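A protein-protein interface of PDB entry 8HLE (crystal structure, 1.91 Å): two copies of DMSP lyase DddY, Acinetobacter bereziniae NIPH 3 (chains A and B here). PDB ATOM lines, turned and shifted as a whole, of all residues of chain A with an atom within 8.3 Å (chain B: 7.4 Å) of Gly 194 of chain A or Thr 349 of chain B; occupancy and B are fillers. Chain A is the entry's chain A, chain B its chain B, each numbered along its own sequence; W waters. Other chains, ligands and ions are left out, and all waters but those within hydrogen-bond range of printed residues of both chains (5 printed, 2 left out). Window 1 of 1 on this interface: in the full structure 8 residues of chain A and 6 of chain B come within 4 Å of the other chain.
The backbone NH of Asp 189 of chain A lies within hydrogen-bond range of the backbone carbonyl oxygen of Gln 348 of chain B (3.2 Å).
The side-chain hydroxyl (OG1) of Thr 349 of chain B lies within hydrogen-bond range of the backbone carbonyl oxygen (O) of Asp 189 of chain A (2.7 Å).
N of Cys 346 of chain B is in hydrogen-bond range of O of Lys 193 of chain A (3.3 Å).
The backbone carbonyl oxygen (O) of Gly 194 of chain A sits close to the side-chain hydroxyl (OG1) of Thr 349 of chain B (3.3 Å).
The side-chain amide oxygen (OE1) of Gln 56 of chain A lies within hydrogen-bond range of the backbone NH (N) of Lys 188 of chain A (3.1 Å).
O of Ser 178 of chain A is in hydrogen-bond range of NZ of Lys 193 of chain A (3.0 Å).
The backbone carbonyl oxygen (O) of Thr 180 of chain A sits at hydrogen-bond distance from the side-chain amino group (NZ) of Lys 193 of chain A, 3.1 Å away.
OD1 of Asp 189 of chain A is in hydrogen-bond range of OG1 of Thr 182 of chain A (3.0 Å).
The side-chain carboxylate (OD1) of Asp 189 of chain A is in hydrogen-bond range of the side-chain hydroxyl (OG) of Ser 191 of chain A, at 3.0 Å.
The side-chain sulfur (SG) of Cys 346 of chain B forms a disulfide with the side-chain sulfur (SG) of Cys 279 of chain B (2.1 Å).
CD1 of Ile 52 of chain A touches CG2 of Thr 349 of chain B, 3.8 Å away.
Gln 348 of chain B touches Lys 188 of chain A.
CD of Lys 188 of chain A touches O of Thr 349 of chain B (3.6 Å).
Lys 193 of chain A touches Gly 345 of chain B.
O of Gly 345 of chain B touches CA of Gly 194 of chain A, 3.9 Å away.
Gly 194 of chain A touches Cys 346 of chain B.
Thr 349 of chain B touches Leu 195 of chain A (CG2 to CD2, 3.6 Å).
CG of Pro 196 of chain A touches CB of Cys 279 of chain B, 3.7 Å away.
Of the printed residues of chain B, Gly 194 of chain A touches Gly 345 (3.9 Å), Cys 346 (3.6 Å) and Thr 349 (3.3 Å).
Of the printed residues of chain B, Ile 52 of chain A touches Thr 349.
Of the printed residues of chain A, Cys 346 of chain B touches Lys 193 and Gly 194.
Of the printed residues of chain A, Gly 345 of chain B touches Lys 193 and Gly 194.
The nearest residue of chain A that does not touch Thr 349 of chain B is Val 190 of chain A (4.8 Å).
The nearest printed residue of chain B that does not touch Ile 52 of chain A is Ile 350 of chain B (6.0 Å).
Printed residues of chain B that touch a printed residue of chain A: Cys 279, Gly 345, Cys 346, Gln 348 and Thr 349.
No position is printed for both chains.
Water W2 bridges OE1 of Gln 278 of chain B (2.6 Å) and NE2 of Gln 45 of chain A (3.1 Å).
Water W3 bridges the side-chain carboxylate of Asp 189 of chain A (2.7 Å) and the backbone carbonyl oxygen of Gly 345 of chain B (2.7 Å).
Water W1 lies within hydrogen-bond range of the backbone carbonyl oxygen of Gln 348 of chain B (2.7 Å) and the backbone carbonyl oxygen of Thr 187 of chain A (3.3 Å).
Water W4 bridges OE2 of Glu 49 of chain A (2.7 Å) and O of Gln 278 of chain B (2.9 Å).
Water W5 lies within hydrogen-bond range of NZ of Lys 188 of chain A (2.8 Å) and O of Thr 349 of chain B (2.9 Å).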
ATOM      1  N   GLN A  45       2.681   4.556 -27.931  1.00  0.00           N
ATOM      2  CA  GLN A  45       1.375   5.014 -27.464  1.00  0.00           C
ATOM      3  C   GLN A  45       0.346   4.974 -28.593  1.00  0.00           C
ATOM      4  O   GLN A  45      -0.800   4.567 -28.382  1.00  0.00           O
ATOM      5  CB  GLN A  45       1.474   6.423 -26.877  1.00  0.00           C
ATOM      6  CG  GLN A  45       0.177   6.892 -26.217  1.00  0.00           C
ATOM      7  CD  GLN A  45      -0.170   6.095 -24.963  1.00  0.00           C
ATOM      8  OE1 GLN A  45       0.712   5.628 -24.248  1.00  0.00           O
ATOM      9  NE2 GLN A  45      -1.461   5.952 -24.689  1.00  0.00           N
ATOM     10  N   ASN A  48      -0.508   1.333 -29.005  1.00  0.00           N
ATOM     11  CA  ASN A  48      -1.311   0.763 -27.926  1.00  0.00           C
ATOM     12  C   ASN A  48      -2.772   1.179 -28.047  1.00  0.00           C
ATOM     13  O   ASN A  48      -3.670   0.347 -27.894  1.00  0.00           O
ATOM     14  CB  ASN A  48      -0.730   1.152 -26.572  1.00  0.00           C
ATOM     15  CG  ASN A  48       0.528   0.357 -26.230  1.00  0.00           C
ATOM     16  OD1 ASN A  48       0.750  -0.750 -26.748  1.00  0.00           O
ATOM     17  ND2 ASN A  48       1.347   0.909 -25.346  1.00  0.00           N
ATOM     18  N   GLU A  49      -3.033   2.453 -28.358  1.00  0.00           N
ATOM     19  CA  GLU A  49      -4.418   2.887 -28.519  1.00  0.00           C
ATOM     20  C   GLU A  49      -5.047   2.320 -29.791  1.00  0.00           C
ATOM     21  O   GLU A  49      -6.264   2.089 -29.830  1.00  0.00           O
ATOM     22  CB  GLU A  49      -4.493   4.414 -28.498  1.00  0.00           C
ATOM     23  CG  GLU A  49      -4.130   4.984 -27.131  1.00  0.00           C
ATOM     24  CD  GLU A  49      -4.268   6.487 -27.065  1.00  0.00           C
ATOM     25  OE1 GLU A  49      -5.040   7.057 -27.868  1.00  0.00           O
ATOM     26  OE2 GLU A  49      -3.580   7.111 -26.223  1.00  0.00           O
ATOM     27  N   ILE A  52      -6.305  -1.000 -28.692  1.00  0.00           N
ATOM     28  CA  ILE A  52      -7.562  -0.905 -27.958  1.00  0.00           C
ATOM     29  C   ILE A  52      -8.725  -0.719 -28.929  1.00  0.00           C
ATOM     30  O   ILE A  52      -9.782  -1.349 -28.788  1.00  0.00           O
ATOM     31  CB  ILE A  52      -7.500   0.238 -26.927  1.00  0.00           C
ATOM     32  CG1 ILE A  52      -6.495  -0.082 -25.814  1.00  0.00           C
ATOM     33  CG2 ILE A  52      -8.888   0.512 -26.333  1.00  0.00           C
ATOM     34  CD1 ILE A  52      -6.340   1.044 -24.816  1.00  0.00           C
ATOM     35  N   TYR A  53      -8.554   0.175 -29.909  1.00  0.00           N
ATOM     36  CA  TYR A  53      -9.576   0.396 -30.933  1.00  0.00           C
ATOM     37  C   TYR A  53      -9.957  -0.904 -31.623  1.00  0.00           C
ATOM     38  O   TYR A  53     -11.139  -1.158 -31.877  1.00  0.00           O
ATOM     39  CB  TYR A  53      -9.051   1.400 -31.961  1.00  0.00           C
ATOM     40  CG  TYR A  53     -10.101   2.148 -32.767  1.00  0.00           C
ATOM     41  CD1 TYR A  53     -10.949   3.064 -32.156  1.00  0.00           C
ATOM     42  CD2 TYR A  53     -10.202   1.971 -34.145  1.00  0.00           C
ATOM     43  CE1 TYR A  53     -11.891   3.761 -32.892  1.00  0.00           C
ATOM     44  CE2 TYR A  53     -11.138   2.674 -34.896  1.00  0.00           C
ATOM     45  CZ  TYR A  53     -11.981   3.570 -34.258  1.00  0.00           C
ATOM     46  OH  TYR A  53     -12.921   4.291 -34.982  1.00  0.00           O
ATOM     47  N   GLN A  56     -11.770  -3.406 -29.080  1.00  0.00           N
ATOM     48  CA  GLN A  56     -13.148  -2.958 -28.936  1.00  0.00           C
ATOM     49  C   GLN A  56     -13.946  -3.189 -30.215  1.00  0.00           C
ATOM     50  O   GLN A  56     -15.136  -3.524 -30.153  1.00  0.00           O
ATOM     51  CB  GLN A  56     -13.190  -1.478 -28.550  1.00  0.00           C
ATOM     52  CG  GLN A  56     -12.633  -1.226 -27.164  1.00  0.00           C
ATOM     53  CD  GLN A  56     -13.510  -1.850 -26.097  1.00  0.00           C
ATOM     54  OE1 GLN A  56     -14.708  -1.590 -26.041  1.00  0.00           O
ATOM     55  NE2 GLN A  56     -12.921  -2.676 -25.250  1.00  0.00           N
ATOM     56  N   THR A 177     -16.563  16.074 -32.202  1.00  0.00           N
ATOM     57  CA  THR A 177     -16.269  14.649 -32.071  1.00  0.00           C
ATOM     58  C   THR A 177     -16.340  14.151 -30.632  1.00  0.00           C
ATOM     59  O   THR A 177     -16.301  12.934 -30.414  1.00  0.00           O
ATOM     60  CB  THR A 177     -14.883  14.312 -32.662  1.00  0.00           C
ATOM     61  OG1 THR A 177     -13.882  15.177 -32.113  1.00  0.00           O
ATOM     62  CG2 THR A 177     -14.882  14.419 -34.194  1.00  0.00           C
ATOM     63  N   SER A 178     -16.465  15.041 -29.652  1.00  0.00           N
ATOM     64  CA  SER A 178     -16.612  14.644 -28.257  1.00  0.00           C
ATOM     65  C   SER A 178     -18.059  14.434 -27.835  1.00  0.00           C
ATOM     66  O   SER A 178     -18.306  14.025 -26.698  1.00  0.00           O
ATOM     67  CB  SER A 178     -15.983  15.696 -27.342  1.00  0.00           C
ATOM     68  OG  SER A 178     -14.602  15.781 -27.603  1.00  0.00           O
ATOM     69  N   THR A 180     -20.343  12.261 -27.870  1.00  0.00           N
ATOM     70  CA  THR A 180     -20.469  10.832 -28.104  1.00  0.00           C
ATOM     71  C   THR A 180     -20.819  10.162 -26.787  1.00  0.00           C
ATOM     72  O   THR A 180     -20.533  10.685 -25.707  1.00  0.00           O
ATOM     73  CB  THR A 180     -19.161  10.221 -28.635  1.00  0.00           C
ATOM     74  OG1 THR A 180     -18.122  10.509 -27.696  1.00  0.00           O
ATOM     75  CG2 THR A 180     -18.769  10.807 -29.997  1.00  0.00           C
ATOM     76  N   THR A 182     -20.401   6.186 -25.532  1.00  0.00           N
ATOM     77  CA  THR A 182     -19.939   4.845 -25.844  1.00  0.00           C
ATOM     78  C   THR A 182     -20.288   3.840 -24.759  1.00  0.00           C
ATOM     79  O   THR A 182     -19.813   2.708 -24.814  1.00  0.00           O
ATOM     80  CB  THR A 182     -18.427   4.850 -26.055  1.00  0.00           C
ATOM     81  OG1 THR A 182     -17.801   5.411 -24.900  1.00  0.00           O
ATOM     82  CG2 THR A 182     -18.063   5.692 -27.271  1.00  0.00           C
ATOM     83  N   THR A 187     -16.852  -1.401 -23.996  1.00  0.00           N
ATOM     84  CA  THR A 187     -16.370  -1.478 -22.621  1.00  0.00           C
ATOM     85  C   THR A 187     -15.232  -0.511 -22.343  1.00  0.00           C
ATOM     86  O   THR A 187     -14.869  -0.322 -21.173  1.00  0.00           O
ATOM     87  CB  THR A 187     -15.939  -2.905 -22.270  1.00  0.00           C
ATOM     88  OG1 THR A 187     -15.010  -3.394 -23.248  1.00  0.00           O
ATOM     89  CG2 THR A 187     -17.154  -3.809 -22.246  1.00  0.00           C
ATOM     90  N   LYS A 188     -14.666   0.101 -23.384  1.00  0.00           N
ATOM     91  CA  LYS A 188     -13.700   1.179 -23.234  1.00  0.00           C
ATOM     92  C   LYS A 188     -14.100   2.299 -24.184  1.00  0.00           C
ATOM     93  O   LYS A 188     -14.585   2.034 -25.290  1.00  0.00           O
ATOM     94  CB  LYS A 188     -12.277   0.712 -23.532  1.00  0.00           C
ATOM     95  CG  LYS A 188     -11.764  -0.360 -22.612  1.00  0.00           C
ATOM     96  CD  LYS A 188     -10.369  -0.781 -23.028  1.00  0.00           C
ATOM     97  CE  LYS A 188      -9.877  -1.918 -22.141  1.00  0.00           C
ATOM     98  NZ  LYS A 188      -8.482  -2.378 -22.435  1.00  0.00           N
ATOM     99  N   ASP A 189     -13.937   3.541 -23.745  1.00  0.00           N
ATOM    100  CA  ASP A 189     -14.317   4.665 -24.594  1.00  0.00           C
ATOM    101  C   ASP A 189     -13.400   4.706 -25.813  1.00  0.00           C
ATOM    102  O   ASP A 189     -12.187   4.908 -25.678  1.00  0.00           O
ATOM    103  CB  ASP A 189     -14.254   5.984 -23.823  1.00  0.00           C
ATOM    104  CG  ASP A 189     -14.809   7.166 -24.631  1.00  0.00           C
ATOM    105  OD1 ASP A 189     -15.343   6.942 -25.733  1.00  0.00           O
ATOM    106  OD2 ASP A 189     -14.739   8.318 -24.160  1.00  0.00           O
ATOM    107  N   VAL A 190     -13.969   4.489 -27.002  1.00  0.00           N
ATOM    108  CA  VAL A 190     -13.191   4.490 -28.242  1.00  0.00           C
ATOM    109  C   VAL A 190     -13.243   5.833 -28.959  1.00  0.00           C
ATOM    110  O   VAL A 190     -12.704   5.956 -30.062  1.00  0.00           O
ATOM    111  CB  VAL A 190     -13.626   3.362 -29.190  1.00  0.00           C
ATOM    112  CG1 VAL A 190     -13.437   2.016 -28.516  1.00  0.00           C
ATOM    113  CG2 VAL A 190     -15.097   3.537 -29.615  1.00  0.00           C
ATOM    114  N   SER A 191     -13.884   6.839 -28.369  1.00  0.00           N
ATOM    115  CA  SER A 191     -13.951   8.152 -28.993  1.00  0.00           C
ATOM    116  C   SER A 191     -12.664   8.932 -28.741  1.00  0.00           C
ATOM    117  O   SER A 191     -11.737   8.460 -28.077  1.00  0.00           O
ATOM    118  CB  SER A 191     -15.156   8.931 -28.464  1.00  0.00           C
ATOM    119  OG  SER A 191     -14.846   9.496 -27.201  1.00  0.00           O
ATOM    120  N   ILE A 192     -12.622  10.152 -29.294  1.00  0.00           N
ATOM    121  CA  ILE A 192     -11.482  11.054 -29.118  1.00  0.00           C
ATOM    122  C   ILE A 192     -11.214  11.327 -27.640  1.00  0.00           C
ATOM    123  O   ILE A 192     -10.066  11.586 -27.246  1.00  0.00           O
ATOM    124  CB  ILE A 192     -11.706  12.355 -29.920  1.00  0.00           C
ATOM    125  CG1 ILE A 192     -10.442  13.230 -29.941  1.00  0.00           C
ATOM    126  CG2 ILE A 192     -12.906  13.177 -29.377  1.00  0.00           C
ATOM    127  CD1 ILE A 192     -10.438  14.270 -31.029  1.00  0.00           C
ATOM    128  N   LYS A 193     -12.250  11.255 -26.799  1.00  0.00           N
ATOM    129  CA  LYS A 193     -12.044  11.498 -25.370  1.00  0.00           C
ATOM    130  C   LYS A 193     -11.262  10.359 -24.735  1.00  0.00           C
ATOM    131  O   LYS A 193     -10.370  10.592 -23.917  1.00  0.00           O
ATOM    132  CB  LYS A 193     -13.386  11.684 -24.660  1.00  0.00           C
ATOM    133  CG  LYS A 193     -14.161  12.918 -25.103  1.00  0.00           C
ATOM    134  CD  LYS A 193     -15.582  12.917 -24.516  1.00  0.00           C
ATOM    135  CE  LYS A 193     -16.397  11.737 -25.045  1.00  0.00           C
ATOM    136  NZ  LYS A 193     -17.825  11.823 -24.647  1.00  0.00           N
ATOM    137  N   GLY A 194     -11.559   9.124 -25.130  1.00  0.00           N
ATOM    138  CA  GLY A 194     -10.950   7.954 -24.527  1.00  0.00           C
ATOM    139  C   GLY A 194      -9.641   7.551 -25.175  1.00  0.00           C
ATOM    140  O   GLY A 194      -8.755   7.031 -24.493  1.00  0.00           O
ATOM    141  N   LEU A 195      -9.514   7.776 -26.487  1.00  0.00           N
ATOM    142  CA  LEU A 195      -8.307   7.456 -27.252  1.00  0.00           C
ATOM    143  C   LEU A 195      -7.781   8.695 -27.978  1.00  0.00           C
ATOM    144  O   LEU A 195      -7.729   8.733 -29.213  1.00  0.00           O
ATOM    145  CB  LEU A 195      -8.580   6.329 -28.248  1.00  0.00           C
ATOM    146  CG  LEU A 195      -9.061   5.010 -27.644  1.00  0.00           C
ATOM    147  CD1 LEU A 195      -9.450   3.995 -28.745  1.00  0.00           C
ATOM    148  CD2 LEU A 195      -7.958   4.446 -26.772  1.00  0.00           C
ATOM    149  N   PRO A 196      -7.342   9.715 -27.237  1.00  0.00           N
ATOM    150  CA  PRO A 196      -6.960  10.980 -27.892  1.00  0.00           C
ATOM    151  C   PRO A 196      -5.689  10.911 -28.728  1.00  0.00           C
ATOM    152  O   PRO A 196      -5.579  11.666 -29.702  1.00  0.00           O
ATOM    153  CB  PRO A 196      -6.793  11.944 -26.706  1.00  0.00           C
ATOM    154  CG  PRO A 196      -6.399  11.059 -25.570  1.00  0.00           C
ATOM    155  CD  PRO A 196      -7.161   9.773 -25.773  1.00  0.00           C
ATOM    156  N   THR A 197      -4.714  10.070 -28.370  1.00  0.00           N
ATOM    157  CA  THR A 197      -3.537   9.916 -29.219  1.00  0.00           C
ATOM    158  C   THR A 197      -3.917   9.323 -30.573  1.00  0.00           C
ATOM    159  O   THR A 197      -3.388   9.732 -31.614  1.00  0.00           O
ATOM    160  CB  THR A 197      -2.493   9.030 -28.530  1.00  0.00           C
ATOM    161  OG1 THR A 197      -2.297   9.471 -27.179  1.00  0.00           O
ATOM    162  CG2 THR A 197      -1.166   9.087 -29.298  1.00  0.00           C
ATOM    163  N   LEU A 198      -4.834   8.354 -30.575  1.00  0.00           N
ATOM    164  CA  LEU A 198      -5.277   7.743 -31.823  1.00  0.00           C
ATOM    165  C   LEU A 198      -5.974   8.757 -32.717  1.00  0.00           C
ATOM    166  O   LEU A 198      -5.609   8.920 -33.890  1.00  0.00           O
ATOM    167  CB  LEU A 198      -6.201   6.566 -31.522  1.00  0.00           C
ATOM    168  CG  LEU A 198      -6.849   5.916 -32.752  1.00  0.00           C
ATOM    169  CD1 LEU A 198      -5.771   5.262 -33.576  1.00  0.00           C
ATOM    170  CD2 LEU A 198      -7.915   4.916 -32.330  1.00  0.00           C
ATOM    171  N   TRP A 199      -6.980   9.454 -32.177  1.00  0.00           N
ATOM    172  CA  TRP A 199      -7.781  10.351 -33.005  1.00  0.00           C
ATOM    173  C   TRP A 199      -6.974  11.555 -33.445  1.00  0.00           C
ATOM    174  O   TRP A 199      -7.200  12.084 -34.538  1.00  0.00           O
ATOM    175  CB  TRP A 199      -9.043  10.792 -32.256  1.00  0.00           C
ATOM    176  CG  TRP A 199     -10.123   9.742 -32.192  1.00  0.00           C
ATOM    177  CD1 TRP A 199     -10.102   8.580 -31.462  1.00  0.00           C
ATOM    178  CD2 TRP A 199     -11.385   9.755 -32.885  1.00  0.00           C
ATOM    179  NE1 TRP A 199     -11.270   7.874 -31.661  1.00  0.00           N
ATOM    180  CE2 TRP A 199     -12.071   8.574 -32.528  1.00  0.00           C
ATOM    181  CE3 TRP A 199     -11.998  10.644 -33.771  1.00  0.00           C
ATOM    182  CZ2 TRP A 199     -13.349   8.263 -33.026  1.00  0.00           C
ATOM    183  CZ3 TRP A 199     -13.275  10.334 -34.262  1.00  0.00           C
ATOM    184  CH2 TRP A 199     -13.927   9.151 -33.888  1.00  0.00           C
ATOM    185  N   PHE B 256      -7.515   5.773 -10.601  1.00  0.00           N
ATOM    186  CA  PHE B 256      -8.130   6.458 -11.726  1.00  0.00           C
ATOM    187  C   PHE B 256      -9.643   6.268 -11.700  1.00  0.00           C
ATOM    188  O   PHE B 256     -10.177   5.355 -11.058  1.00  0.00           O
ATOM    189  CB  PHE B 256      -7.561   5.952 -13.062  1.00  0.00           C
ATOM    190  CG  PHE B 256      -8.081   4.590 -13.475  1.00  0.00           C
ATOM    191  CD1 PHE B 256      -7.660   3.440 -12.817  1.00  0.00           C
ATOM    192  CD2 PHE B 256      -9.006   4.466 -14.509  1.00  0.00           C
ATOM    193  CE1 PHE B 256      -8.136   2.165 -13.206  1.00  0.00           C
ATOM    194  CE2 PHE B 256      -9.496   3.219 -14.887  1.00  0.00           C
ATOM    195  CZ  PHE B 256      -9.059   2.060 -14.240  1.00  0.00           C
ATOM    196  N   GLN B 278      -1.406   9.524 -19.312  1.00  0.00           N
ATOM    197  CA  GLN B 278      -1.606   8.844 -20.590  1.00  0.00           C
ATOM    198  C   GLN B 278      -2.480   9.645 -21.541  1.00  0.00           C
ATOM    199  O   GLN B 278      -2.575   9.299 -22.731  1.00  0.00           O
ATOM    200  CB  GLN B 278      -2.220   7.454 -20.361  1.00  0.00           C
ATOM    201  CG  GLN B 278      -1.288   6.515 -19.610  1.00  0.00           C
ATOM    202  CD  GLN B 278      -1.975   5.267 -19.072  1.00  0.00           C
ATOM    203  OE1 GLN B 278      -2.330   4.364 -19.833  1.00  0.00           O
ATOM    204  NE2 GLN B 278      -2.147   5.203 -17.747  1.00  0.00           N
ATOM    205  N   CYS B 279      -3.125  10.696 -21.038  1.00  0.00           N
ATOM    206  CA  CYS B 279      -3.814  11.685 -21.845  1.00  0.00           C
ATOM    207  C   CYS B 279      -3.678  12.988 -21.084  1.00  0.00           C
ATOM    208  O   CYS B 279      -3.485  12.975 -19.867  1.00  0.00           O
ATOM    209  CB  CYS B 279      -5.290  11.331 -22.066  1.00  0.00           C
ATOM    210  SG  CYS B 279      -6.216  10.981 -20.544  1.00  0.00           S
ATOM    211  N   ASP B 281      -5.601  15.130 -20.014  1.00  0.00           N
ATOM    212  CA  ASP B 281      -6.587  15.394 -18.969  1.00  0.00           C
ATOM    213  C   ASP B 281      -6.789  14.218 -18.014  1.00  0.00           C
ATOM    214  O   ASP B 281      -7.817  14.152 -17.331  1.00  0.00           O
ATOM    215  CB  ASP B 281      -7.926  15.803 -19.584  1.00  0.00           C
ATOM    216  CG  ASP B 281      -8.448  14.817 -20.622  1.00  0.00           C
ATOM    217  OD1 ASP B 281      -7.661  14.029 -21.188  1.00  0.00           O
ATOM    218  OD2 ASP B 281      -9.672  14.858 -20.902  1.00  0.00           O
ATOM    219  N   GLU B 344     -12.032  12.300 -16.371  1.00  0.00           N
ATOM    220  CA  GLU B 344     -12.144  12.747 -17.755  1.00  0.00           C
ATOM    221  C   GLU B 344     -11.333  11.879 -18.718  1.00  0.00           C
ATOM    222  O   GLU B 344     -10.387  11.195 -18.339  1.00  0.00           O
ATOM    223  CB  GLU B 344     -11.689  14.203 -17.885  1.00  0.00           C
ATOM    224  CG  GLU B 344     -12.408  15.137 -16.945  1.00  0.00           C
ATOM    225  CD  GLU B 344     -13.910  15.021 -17.084  1.00  0.00           C
ATOM    226  OE1 GLU B 344     -14.407  15.156 -18.224  1.00  0.00           O
ATOM    227  OE2 GLU B 344     -14.588  14.776 -16.068  1.00  0.00           O
ATOM    228  N   GLY B 345     -11.711  11.941 -19.988  1.00  0.00           N
ATOM    229  CA  GLY B 345     -10.814  11.487 -21.037  1.00  0.00           C
ATOM    230  C   GLY B 345     -10.508  10.004 -20.945  1.00  0.00           C
ATOM    231  O   GLY B 345     -11.406   9.170 -20.807  1.00  0.00           O
ATOM    232  N   CYS B 346      -9.214   9.683 -20.986  1.00  0.00           N
ATOM    233  CA  CYS B 346      -8.734   8.311 -21.055  1.00  0.00           C
ATOM    234  C   CYS B 346      -8.902   7.552 -19.746  1.00  0.00           C
ATOM    235  O   CYS B 346      -8.636   6.349 -19.724  1.00  0.00           O
ATOM    236  CB  CYS B 346      -7.260   8.287 -21.493  1.00  0.00           C
ATOM    237  SG  CYS B 346      -6.081   8.947 -20.291  1.00  0.00           S
ATOM    238  N   ASN B 347      -9.336   8.206 -18.666  1.00  0.00           N
ATOM    239  CA  ASN B 347      -9.745   7.455 -17.482  1.00  0.00           C
ATOM    240  C   ASN B 347     -10.880   6.490 -17.793  1.00  0.00           C
ATOM    241  O   ASN B 347     -11.073   5.514 -17.054  1.00  0.00           O
ATOM    242  CB  ASN B 347     -10.164   8.401 -16.353  1.00  0.00           C
ATOM    243  CG  ASN B 347      -8.983   9.135 -15.736  1.00  0.00           C
ATOM    244  OD1 ASN B 347      -8.180   8.547 -14.999  1.00  0.00           O
ATOM    245  ND2 ASN B 347      -8.887  10.429 -16.009  1.00  0.00           N
ATOM    246  N   GLN B 348     -11.618   6.730 -18.884  1.00  0.00           N
ATOM    247  CA  GLN B 348     -12.671   5.831 -19.334  1.00  0.00           C
ATOM    248  C   GLN B 348     -12.151   4.712 -20.236  1.00  0.00           C
ATOM    249  O   GLN B 348     -12.954   3.929 -20.766  1.00  0.00           O
ATOM    250  CB  GLN B 348     -13.765   6.628 -20.055  1.00  0.00           C
ATOM    251  CG  GLN B 348     -14.467   7.666 -19.167  1.00  0.00           C
ATOM    252  CD  GLN B 348     -14.749   7.142 -17.766  1.00  0.00           C
ATOM    253  OE1 GLN B 348     -15.322   6.065 -17.595  1.00  0.00           O
ATOM    254  NE2 GLN B 348     -14.345   7.907 -16.756  1.00  0.00           N
ATOM    255  N   THR B 349     -10.833   4.613 -20.408  1.00  0.00           N
ATOM    256  CA  THR B 349     -10.245   3.636 -21.319  1.00  0.00           C
ATOM    257  C   THR B 349      -9.067   2.908 -20.674  1.00  0.00           C
ATOM    258  O   THR B 349      -8.850   1.719 -20.934  1.00  0.00           O
ATOM    259  CB  THR B 349      -9.813   4.333 -22.612  1.00  0.00           C
ATOM    260  OG1 THR B 349     -10.974   4.873 -23.263  1.00  0.00           O
ATOM    261  CG2 THR B 349      -9.147   3.354 -23.556  1.00  0.00           C
ATOM    262  N   ILE B 350      -8.330   3.587 -19.792  1.00  0.00           N
ATOM    263  CA  ILE B 350      -7.091   3.033 -19.244  1.00  0.00           C
ATOM    264  C   ILE B 350      -7.375   2.012 -18.148  1.00  0.00           C
ATOM    265  O   ILE B 350      -8.522   1.826 -17.723  1.00  0.00           O
ATOM    266  CB  ILE B 350      -6.158   4.148 -18.726  1.00  0.00           C
ATOM    267  CG1 ILE B 350      -6.828   4.930 -17.579  1.00  0.00           C
ATOM    268  CG2 ILE B 350      -5.718   5.081 -19.874  1.00  0.00           C
ATOM    269  CD1 ILE B 350      -6.139   6.278 -17.244  1.00  0.00           C
ATOM    270  N   LYS B 351      -6.322   1.331 -17.692  1.00  0.00           N
ATOM    271  CA  LYS B 351      -6.413   0.366 -16.608  1.00  0.00           C
ATOM    272  C   LYS B 351      -5.204   0.542 -15.699  1.00  0.00           C
ATOM    273  O   LYS B 351      -4.181   1.087 -16.111  1.00  0.00           O
ATOM    274  CB  LYS B 351      -6.500  -1.082 -17.145  1.00  0.00           C
ATOM    275  CG  LYS B 351      -7.940  -1.508 -17.411  1.00  0.00           C
ATOM    276  CD  LYS B 351      -8.740  -1.424 -16.116  1.00  0.00           C
ATOM    277  CE  LYS B 351     -10.185  -0.996 -16.276  1.00  0.00           C
ATOM    278  NZ  LYS B 351     -10.941  -1.389 -17.482  1.00  0.00           N
HETATM  279  O   HOH W   1     -14.867   2.488 -19.501  1.00  0.00           O
HETATM  280  O   HOH W   2      -2.325   4.122 -22.399  1.00  0.00           O
HETATM  281  O   HOH W   3     -13.859   9.557 -21.977  1.00  0.00           O
HETATM  282  O   HOH W   4      -4.852   7.978 -23.991  1.00  0.00           O
HETATM  283  O   HOH W   5      -6.909  -0.379 -21.354  1.00  0.00           O
